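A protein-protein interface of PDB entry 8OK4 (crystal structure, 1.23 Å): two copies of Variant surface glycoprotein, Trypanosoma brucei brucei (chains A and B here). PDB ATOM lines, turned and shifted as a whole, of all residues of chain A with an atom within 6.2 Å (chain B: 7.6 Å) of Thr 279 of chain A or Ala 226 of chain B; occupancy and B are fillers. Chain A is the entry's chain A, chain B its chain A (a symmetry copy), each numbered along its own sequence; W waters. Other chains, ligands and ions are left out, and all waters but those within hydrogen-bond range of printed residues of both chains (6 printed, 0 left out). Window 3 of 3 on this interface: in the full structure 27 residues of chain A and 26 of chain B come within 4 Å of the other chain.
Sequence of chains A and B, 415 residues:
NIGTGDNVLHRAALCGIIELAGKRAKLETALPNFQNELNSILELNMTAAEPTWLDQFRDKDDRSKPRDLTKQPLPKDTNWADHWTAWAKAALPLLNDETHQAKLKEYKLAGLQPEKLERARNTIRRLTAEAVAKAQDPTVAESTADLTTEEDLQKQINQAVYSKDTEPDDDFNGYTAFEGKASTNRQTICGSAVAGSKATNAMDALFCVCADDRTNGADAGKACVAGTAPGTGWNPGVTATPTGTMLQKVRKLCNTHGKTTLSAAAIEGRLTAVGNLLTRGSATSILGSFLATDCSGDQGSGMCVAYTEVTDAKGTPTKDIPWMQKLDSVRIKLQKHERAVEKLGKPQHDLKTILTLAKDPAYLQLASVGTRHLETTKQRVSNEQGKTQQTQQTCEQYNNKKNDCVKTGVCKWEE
O of Asn 276 of chain A sits at hydrogen-bond distance from NH2 of Arg 11 of chain B.
The guanidinium group of Arg 11 of chain B is in hydrogen-bond range of the backbone carbonyl oxygen of Leu 277 of chain A, at 3.1 Å.
The backbone carbonyl oxygen of Leu 278 of chain A sits at hydrogen-bond distance from the guanidinium group of Arg 11 of chain B, at 3.3 Å.
OG1 of Thr 279 of chain A is in hydrogen-bond range of NH1 of Arg 11 of chain B (2.8 Å).
The backbone carbonyl oxygen (O) of Leu 277 of chain A is in hydrogen-bond range of the side-chain hydroxyl (OG1) of Thr 279 of chain A, at 3.5 Å.
The backbone NH of Thr 279 of chain A sits at hydrogen-bond distance from the backbone carbonyl oxygen of Ile 286 of chain A, 2.8 Å away.
O of Cys 224 of chain B lies within hydrogen-bond range of NH1 of Arg 11 of chain B (3.0 Å).
The side-chain amino group of Lys 222 of chain B sits close to the backbone carbonyl oxygen of Gly 227 of chain B.
Thr 279 of chain A touches Cys 224 of chain B (CG2 to O, 3.9 Å).
Val 225 of chain B touches Thr 279 of chain A.
Thr 279 of chain A touches Ala 226 of chain B (CG2 to N, 3.4 Å).
Lys 252 of chain B touches Arg 280 of chain A (O to CD, 3.97 Å).
O of Leu 253 of chain B touches CD of Arg 280 of chain A, 3.5 Å away.
CG2 of Thr 4 of chain B touches O of Phe 290 of chain A (3.4 Å).
Phe 290 of chain A touches Ala 226 of chain B (CD1 to CB, 3.5 Å).
Gly 227 of chain B touches Phe 290 of chain A (N to CD1, 3.8 Å).
CD2 of Leu 291 of chain A touches CB of Thr 4 of chain B (3.9 Å).
Of the printed residues of chain B, Leu 278 of chain A touches Arg 11.
Printed residues of chain B within 4 Å of Thr 279 of chain A: Arg 11 (2.8 Å), Cys 224 (3.9 Å), Val 225 (3.6 Å) and Ala 226 (3.4 Å).
Of the printed residues of chain B, Phe 290 of chain A touches Thr 4, Ala 226 and Gly 227.
Of the printed residues of chain A, Thr 4 of chain B touches Phe 290 and Leu 291.
Of chain A, only Thr 279 and Phe 290 come within 4 Å of Ala 226 of chain B.
Of the printed residues of chain A, Gly 227 of chain B touches Phe 290 (3.8 Å).
The nearest residue of chain A that does not touch Ala 226 of chain B is Ile 286 of chain A (4.2 Å).
Of the 16 printed residues of chain A, 7 touch a printed residue of chain B.
Printed residues of chain A that touch a printed residue of chain B: Asn 276, Leu 277, Leu 278, Thr 279, Arg 280, Phe 290 and Leu 291.
Hydrophobic or aromatic side chains of chain A within 4 Å of the printed part of chain B: Phe 290 and Leu 291.
Of the 14 printed residues of chain B, 8 touch a printed residue of chain A.
No position is printed for both chains.
Water W6 bridges the backbone carbonyl oxygen (O) of Leu 291 of chain A and the side-chain hydroxyl (OG1) of Thr 4 of chain B.
Water W4 lies within hydrogen-bond range of O of Asn 276 of chain A and NE of Arg 11 of chain B.
Water W5 lies within hydrogen-bond range of O of Leu 253 of chain B (2.7 Å), N of Arg 280 of chain A (2.8 Å), O of Leu 278 of chain A (2.9 Å) and NE of Arg 11 of chain B (3.3 Å).
Water W1 bridges O of Val 225 of chain B (2.8 Å) and O of Phe 290 of chain A (3.0 Å).
Water W2 lies within hydrogen-bond range of the backbone carbonyl oxygen of Leu 253 of chain B (3.0 Å) and the side-chain amide nitrogen of Asn 276 of chain A (3.4 Å).
Water W3 bridges the backbone NH (N) of Ala 226 of chain B (3.1 Å) and the backbone carbonyl oxygen (O) of Arg 280 of chain A (3.2 Å).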
ATOM      1  N   ALA A 193      28.730  19.649 -18.244  1.00  0.00           N
ATOM      2  CA  ALA A 193      29.226  20.976 -18.570  1.00  0.00           C
ATOM      3  C   ALA A 193      30.653  20.947 -19.094  1.00  0.00           C
ATOM      4  O   ALA A 193      31.126  21.962 -19.610  1.00  0.00           O
ATOM      5  CB  ALA A 193      29.166  21.871 -17.328  1.00  0.00           C
ATOM      6  N   GLY A 275      18.387  23.276 -32.978  1.00  0.00           N
ATOM      7  CA  GLY A 275      19.657  23.977 -32.902  1.00  0.00           C
ATOM      8  C   GLY A 275      19.658  25.118 -31.903  1.00  0.00           C
ATOM      9  O   GLY A 275      20.641  25.331 -31.195  1.00  0.00           O
ATOM     10  N   ASN A 276      18.575  25.885 -31.853  1.00  0.00           N
ATOM     11  CA  ASN A 276      18.520  27.032 -30.958  1.00  0.00           C
ATOM     12  C   ASN A 276      18.123  26.645 -29.540  1.00  0.00           C
ATOM     13  O   ASN A 276      18.302  27.456 -28.627  1.00  0.00           O
ATOM     14  CB  ASN A 276      17.580  28.094 -31.524  1.00  0.00           C
ATOM     15  CG  ASN A 276      18.186  28.839 -32.709  1.00  0.00           C
ATOM     16  OD1 ASN A 276      17.593  28.912 -33.779  1.00  0.00           O
ATOM     17  ND2 ASN A 276      19.377  29.375 -32.522  1.00  0.00           N
ATOM     18  N   LEU A 277      17.639  25.421 -29.319  1.00  0.00           N
ATOM     19  CA  LEU A 277      17.446  24.944 -27.956  1.00  0.00           C
ATOM     20  C   LEU A 277      18.761  24.560 -27.294  1.00  0.00           C
ATOM     21  O   LEU A 277      18.806  24.461 -26.067  1.00  0.00           O
ATOM     22  CB  LEU A 277      16.486  23.757 -27.924  1.00  0.00           C
ATOM     23  CG  LEU A 277      15.014  24.116 -28.110  1.00  0.00           C
ATOM     24  CD1 LEU A 277      14.205  22.822 -28.193  1.00  0.00           C
ATOM     25  CD2 LEU A 277      14.456  25.010 -27.020  1.00  0.00           C
ATOM     26  N   LEU A 278      19.823  24.344 -28.068  1.00  0.00           N
ATOM     27  CA  LEU A 278      21.121  24.048 -27.479  1.00  0.00           C
ATOM     28  C   LEU A 278      21.601  25.233 -26.655  1.00  0.00           C
ATOM     29  O   LEU A 278      21.774  26.336 -27.179  1.00  0.00           O
ATOM     30  CB  LEU A 278      22.144  23.723 -28.563  1.00  0.00           C
ATOM     31  CG  LEU A 278      22.055  22.323 -29.158  1.00  0.00           C
ATOM     32  CD1 LEU A 278      22.701  22.273 -30.539  1.00  0.00           C
ATOM     33  CD2 LEU A 278      22.692  21.313 -28.223  1.00  0.00           C
ATOM     34  N   THR A 279      21.835  24.989 -25.370  1.00  0.00           N
ATOM     35  CA  THR A 279      22.253  26.017 -24.417  1.00  0.00           C
ATOM     36  C   THR A 279      23.774  26.056 -24.394  1.00  0.00           C
ATOM     37  O   THR A 279      24.419  25.119 -23.911  1.00  0.00           O
ATOM     38  CB  THR A 279      21.672  25.683 -23.044  1.00  0.00           C
ATOM     39  OG1 THR A 279      20.238  25.653 -23.152  1.00  0.00           O
ATOM     40  CG2 THR A 279      22.118  26.701 -21.971  1.00  0.00           C
ATOM     41  N   ARG A 280      24.344  27.136 -24.928  1.00  0.00           N
ATOM     42  CA  ARG A 280      25.783  27.214 -25.160  1.00  0.00           C
ATOM     43  C   ARG A 280      26.526  27.650 -23.901  1.00  0.00           C
ATOM     44  O   ARG A 280      26.264  28.727 -23.356  1.00  0.00           O
ATOM     45  CB  ARG A 280      26.078  28.192 -26.296  1.00  0.00           C
ATOM     46  CG  ARG A 280      25.591  27.711 -27.654  1.00  0.00           C
ATOM     47  CD  ARG A 280      25.768  28.771 -28.732  1.00  0.00           C
ATOM     48  NE  ARG A 280      25.383  28.280 -30.051  1.00  0.00           N
ATOM     49  CZ  ARG A 280      26.213  28.015 -31.054  1.00  0.00           C
ATOM     50  NH1 ARG A 280      27.526  28.137 -30.926  1.00  0.00           N
ATOM     51  NH2 ARG A 280      25.711  27.606 -32.218  1.00  0.00           N
ATOM     52  N   GLY A 281      27.482  26.828 -23.473  1.00  0.00           N
ATOM     53  CA  GLY A 281      28.359  27.150 -22.366  1.00  0.00           C
ATOM     54  C   GLY A 281      29.809  27.198 -22.809  1.00  0.00           C
ATOM     55  O   GLY A 281      30.115  27.184 -24.011  1.00  0.00           O
ATOM     56  N   THR A 284      30.725  22.989 -23.463  1.00  0.00           N
ATOM     57  CA  THR A 284      29.739  22.177 -24.144  1.00  0.00           C
ATOM     58  C   THR A 284      28.481  23.006 -24.331  1.00  0.00           C
ATOM     59  O   THR A 284      28.317  24.078 -23.734  1.00  0.00           O
ATOM     60  CB  THR A 284      29.338  20.929 -23.336  1.00  0.00           C
ATOM     61  OG1 THR A 284      28.683  21.342 -22.126  1.00  0.00           O
ATOM     62  CG2 THR A 284      30.534  20.061 -23.009  1.00  0.00           C
ATOM     63  N   SER A 285      27.585  22.487 -25.162  1.00  0.00           N
ATOM     64  CA  SER A 285      26.220  22.972 -25.245  1.00  0.00           C
ATOM     65  C   SER A 285      25.275  21.841 -24.876  1.00  0.00           C
ATOM     66  O   SER A 285      25.511  20.677 -25.223  1.00  0.00           O
ATOM     67  CB  SER A 285      25.891  23.491 -26.634  1.00  0.00           C
ATOM     68  OG  SER A 285      26.739  24.567 -26.989  1.00  0.00           O
ATOM     69  N   ILE A 286      24.186  22.201 -24.211  1.00  0.00           N
ATOM     70  CA  ILE A 286      23.301  21.253 -23.553  1.00  0.00           C
ATOM     71  C   ILE A 286      21.918  21.332 -24.174  1.00  0.00           C
ATOM     72  O   ILE A 286      21.336  22.418 -24.267  1.00  0.00           O
ATOM     73  CB  ILE A 286      23.185  21.557 -22.048  1.00  0.00           C
ATOM     74  CG1 ILE A 286      24.552  21.582 -21.370  1.00  0.00           C
ATOM     75  CG2 ILE A 286      22.258  20.539 -21.404  1.00  0.00           C
ATOM     76  CD1 ILE A 286      25.199  20.247 -21.233  1.00  0.00           C
ATOM     77  N   LEU A 287      21.355  20.171 -24.504  1.00  0.00           N
ATOM     78  CA  LEU A 287      19.969  20.050 -24.934  1.00  0.00           C
ATOM     79  C   LEU A 287      19.201  19.316 -23.845  1.00  0.00           C
ATOM     80  O   LEU A 287      19.501  18.156 -23.546  1.00  0.00           O
ATOM     81  CB  LEU A 287      19.873  19.275 -26.245  1.00  0.00           C
ATOM     82  CG  LEU A 287      18.466  19.100 -26.811  1.00  0.00           C
ATOM     83  CD1 LEU A 287      17.864  20.454 -27.156  1.00  0.00           C
ATOM     84  CD2 LEU A 287      18.535  18.212 -28.042  1.00  0.00           C
ATOM     85  N   GLY A 288      18.220  19.991 -23.257  1.00  0.00           N
ATOM     86  CA  GLY A 288      17.456  19.431 -22.162  1.00  0.00           C
ATOM     87  C   GLY A 288      17.589  20.238 -20.894  1.00  0.00           C
ATOM     88  O   GLY A 288      18.509  21.054 -20.755  1.00  0.00           O
ATOM     89  N   PHE A 290      18.669  21.418 -17.428  1.00  0.00           N
ATOM     90  CA  PHE A 290      19.963  21.300 -16.777  1.00  0.00           C
ATOM     91  C   PHE A 290      20.014  22.331 -15.669  1.00  0.00           C
ATOM     92  O   PHE A 290      19.788  23.520 -15.911  1.00  0.00           O
ATOM     93  CB  PHE A 290      21.092  21.550 -17.775  1.00  0.00           C
ATOM     94  CG  PHE A 290      22.482  21.472 -17.178  1.00  0.00           C
ATOM     95  CD1 PHE A 290      22.957  22.461 -16.322  1.00  0.00           C
ATOM     96  CD2 PHE A 290      23.320  20.412 -17.485  1.00  0.00           C
ATOM     97  CE1 PHE A 290      24.236  22.395 -15.804  1.00  0.00           C
ATOM     98  CE2 PHE A 290      24.597  20.343 -16.961  1.00  0.00           C
ATOM     99  CZ  PHE A 290      25.056  21.338 -16.130  1.00  0.00           C
ATOM    100  N   LEU A 291      20.313  21.869 -14.463  1.00  0.00           N
ATOM    101  CA  LEU A 291      20.439  22.735 -13.304  1.00  0.00           C
ATOM    102  C   LEU A 291      21.858  22.803 -12.774  1.00  0.00           C
ATOM    103  O   LEU A 291      22.302  23.873 -12.354  1.00  0.00           O
ATOM    104  CB  LEU A 291      19.521  22.242 -12.177  1.00  0.00           C
ATOM    105  CG  LEU A 291      18.022  22.216 -12.478  1.00  0.00           C
ATOM    106  CD1 LEU A 291      17.247  21.723 -11.262  1.00  0.00           C
ATOM    107  CD2 LEU A 291      17.517  23.580 -12.909  1.00  0.00           C
ATOM    108  N   ALA A 292      22.586  21.688 -12.770  1.00  0.00           N
ATOM    109  CA  ALA A 292      23.898  21.684 -12.142  1.00  0.00           C
ATOM    110  C   ALA A 292      24.743  20.534 -12.661  1.00  0.00           C
ATOM    111  O   ALA A 292      24.276  19.391 -12.734  1.00  0.00           O
ATOM    112  CB  ALA A 292      23.768  21.566 -10.618  1.00  0.00           C
ATOM    113  N   THR B   4      17.089  28.579 -13.018  1.00  0.00           N
ATOM    114  CA  THR B   4      17.940  28.118 -14.108  1.00  0.00           C
ATOM    115  C   THR B   4      17.118  27.510 -15.239  1.00  0.00           C
ATOM    116  O   THR B   4      16.287  26.624 -15.022  1.00  0.00           O
ATOM    117  CB  THR B   4      18.948  27.105 -13.559  1.00  0.00           C
ATOM    118  OG1 THR B   4      19.695  27.695 -12.487  1.00  0.00           O
ATOM    119  CG2 THR B   4      19.912  26.649 -14.634  1.00  0.00           C
ATOM    120  N   GLY B   5      17.346  28.012 -16.452  1.00  0.00           N
ATOM    121  CA  GLY B   5      16.747  27.467 -17.654  1.00  0.00           C
ATOM    122  C   GLY B   5      15.320  27.885 -17.932  1.00  0.00           C
ATOM    123  O   GLY B   5      14.756  27.460 -18.949  1.00  0.00           O
ATOM    124  N   VAL B   8      14.792  29.305 -21.480  1.00  0.00           N
ATOM    125  CA  VAL B   8      15.392  28.646 -22.644  1.00  0.00           C
ATOM    126  C   VAL B   8      14.493  28.798 -23.877  1.00  0.00           C
ATOM    127  O   VAL B   8      14.972  29.053 -24.989  1.00  0.00           O
ATOM    128  CB  VAL B   8      15.734  27.179 -22.314  1.00  0.00           C
ATOM    129  CG1 VAL B   8      16.029  26.372 -23.573  1.00  0.00           C
ATOM    130  CG2 VAL B   8      16.934  27.115 -21.367  1.00  0.00           C
ATOM    131  N   ARG B  11      14.873  32.484 -25.113  1.00  0.00           N
ATOM    132  CA  ARG B  11      16.212  32.648 -25.654  1.00  0.00           C
ATOM    133  C   ARG B  11      16.311  32.001 -27.024  1.00  0.00           C
ATOM    134  O   ARG B  11      16.853  32.591 -27.966  1.00  0.00           O
ATOM    135  CB  ARG B  11      17.230  32.028 -24.700  1.00  0.00           C
ATOM    136  CG  ARG B  11      18.670  32.187 -25.157  1.00  0.00           C
ATOM    137  CD  ARG B  11      19.528  31.020 -24.689  1.00  0.00           C
ATOM    138  NE  ARG B  11      19.242  29.786 -25.413  1.00  0.00           N
ATOM    139  CZ  ARG B  11      19.270  28.565 -24.891  1.00  0.00           C
ATOM    140  NH1 ARG B  11      19.515  28.365 -23.606  1.00  0.00           N
ATOM    141  NH2 ARG B  11      19.065  27.517 -25.685  1.00  0.00           N
ATOM    142  N   LYS B 222      20.174  33.005 -14.090  1.00  0.00           N
ATOM    143  CA  LYS B 222      20.489  31.787 -14.823  1.00  0.00           C
ATOM    144  C   LYS B 222      19.364  31.370 -15.773  1.00  0.00           C
ATOM    145  O   LYS B 222      19.409  30.275 -16.337  1.00  0.00           O
ATOM    146  CB  LYS B 222      20.792  30.666 -13.831  1.00  0.00           C
ATOM    147  CG  LYS B 222      22.099  30.842 -13.066  1.00  0.00           C
ATOM    148  CD  LYS B 222      22.428  29.588 -12.253  1.00  0.00           C
ATOM    149  CE  LYS B 222      23.643  29.798 -11.370  1.00  0.00           C
ATOM    150  NZ  LYS B 222      24.060  28.547 -10.656  1.00  0.00           N
ATOM    151  N   ALA B 223      18.369  32.230 -15.980  1.00  0.00           N
ATOM    152  CA  ALA B 223      17.195  31.844 -16.763  1.00  0.00           C
ATOM    153  C   ALA B 223      17.532  31.334 -18.164  1.00  0.00           C
ATOM    154  O   ALA B 223      16.815  30.468 -18.682  1.00  0.00           O
ATOM    155  CB  ALA B 223      16.228  33.020 -16.848  1.00  0.00           C
ATOM    156  N   CYS B 224      18.574  31.853 -18.802  1.00  0.00           N
ATOM    157  CA  CYS B 224      18.881  31.482 -20.178  1.00  0.00           C
ATOM    158  C   CYS B 224      20.036  30.508 -20.314  1.00  0.00           C
ATOM    159  O   CYS B 224      20.405  30.177 -21.446  1.00  0.00           O
ATOM    160  CB  CYS B 224      19.182  32.733 -21.002  1.00  0.00           C
ATOM    161  SG  CYS B 224      17.709  33.797 -21.111  1.00  0.00           S
ATOM    162  N   VAL B 225      20.609  30.035 -19.205  1.00  0.00           N
ATOM    163  CA  VAL B 225      21.850  29.275 -19.258  1.00  0.00           C
ATOM    164  C   VAL B 225      21.672  27.910 -18.616  1.00  0.00           C
ATOM    165  O   VAL B 225      20.587  27.576 -18.127  1.00  0.00           O
ATOM    166  CB  VAL B 225      23.025  30.040 -18.615  1.00  0.00           C
ATOM    167  CG1 VAL B 225      23.291  31.343 -19.365  1.00  0.00           C
ATOM    168  CG2 VAL B 225      22.762  30.311 -17.145  1.00  0.00           C
ATOM    169  N   ALA B 226      22.735  27.110 -18.661  1.00  0.00           N
ATOM    170  CA  ALA B 226      22.805  25.800 -18.023  1.00  0.00           C
ATOM    171  C   ALA B 226      23.925  25.921 -17.001  1.00  0.00           C
ATOM    172  O   ALA B 226      25.107  25.860 -17.358  1.00  0.00           O
ATOM    173  CB  ALA B 226      23.090  24.700 -19.040  1.00  0.00           C
ATOM    174  N   GLY B 227      23.555  26.144 -15.746  1.00  0.00           N
ATOM    175  CA  GLY B 227      24.533  26.312 -14.695  1.00  0.00           C
ATOM    176  C   GLY B 227      25.036  27.736 -14.605  1.00  0.00           C
ATOM    177  O   GLY B 227      24.343  28.616 -14.096  1.00  0.00           O
ATOM    178  N   THR B 228      26.229  27.976 -15.135  1.00  0.00           N
ATOM    179  CA  THR B 228      26.926  29.238 -14.916  1.00  0.00           C
ATOM    180  C   THR B 228      26.164  30.424 -15.499  1.00  0.00           C
ATOM    181  O   THR B 228      25.876  30.453 -16.695  1.00  0.00           O
ATOM    182  CB  THR B 228      28.303  29.128 -15.573  1.00  0.00           C
ATOM    183  OG1 THR B 228      28.889  27.855 -15.259  1.00  0.00           O
ATOM    184  CG2 THR B 228      29.197  30.252 -15.111  1.00  0.00           C
ATOM    185  N   ALA B 229      25.882  31.431 -14.660  1.00  0.00           N
ATOM    186  CA  ALA B 229      25.265  32.667 -15.137  1.00  0.00           C
ATOM    187  C   ALA B 229      26.216  33.394 -16.089  1.00  0.00           C
ATOM    188  O   ALA B 229      27.430  33.185 -16.033  1.00  0.00           O
ATOM    189  CB  ALA B 229      24.938  33.578 -13.952  1.00  0.00           C
ATOM    190  N   LYS B 252      26.651  35.804 -26.990  1.00  0.00           N
ATOM    191  CA  LYS B 252      27.337  34.546 -27.264  1.00  0.00           C
ATOM    192  C   LYS B 252      26.508  33.325 -26.900  1.00  0.00           C
ATOM    193  O   LYS B 252      26.962  32.201 -27.140  1.00  0.00           O
ATOM    194  CB  LYS B 252      28.703  34.511 -26.585  1.00  0.00           C
ATOM    195  CG  LYS B 252      28.661  34.327 -25.095  1.00  0.00           C
ATOM    196  CD  LYS B 252      30.055  34.521 -24.517  1.00  0.00           C
ATOM    197  CE  LYS B 252      30.096  34.224 -23.041  1.00  0.00           C
ATOM    198  NZ  LYS B 252      31.457  34.475 -22.500  1.00  0.00           N
ATOM    199  N   LEU B 253      25.309  33.504 -26.345  1.00  0.00           N
ATOM    200  CA  LEU B 253      24.380  32.385 -26.237  1.00  0.00           C
ATOM    201  C   LEU B 253      23.785  32.001 -27.589  1.00  0.00           C
ATOM    202  O   LEU B 253      23.210  30.911 -27.712  1.00  0.00           O
ATOM    203  CB  LEU B 253      23.243  32.737 -25.281  1.00  0.00           C
ATOM    204  CG  LEU B 253      23.684  33.046 -23.852  1.00  0.00           C
ATOM    205  CD1 LEU B 253      22.503  33.507 -23.028  1.00  0.00           C
ATOM    206  CD2 LEU B 253      24.354  31.838 -23.203  1.00  0.00           C
HETATM  207  O   HOH W   1      19.419  25.088 -18.416  1.00  0.00           O
HETATM  208  O   HOH W   2      21.509  29.792 -29.855  1.00  0.00           O
HETATM  209  O   HOH W   3      25.153  27.866 -20.510  1.00  0.00           O
HETATM  210  O   HOH W   4      19.494  29.828 -28.239  1.00  0.00           O
HETATM  211  O   HOH W   5      22.421  28.916 -26.002  1.00  0.00           O
HETATM  212  O   HOH W   6      21.194  25.929 -11.100  1.00  0.00           O
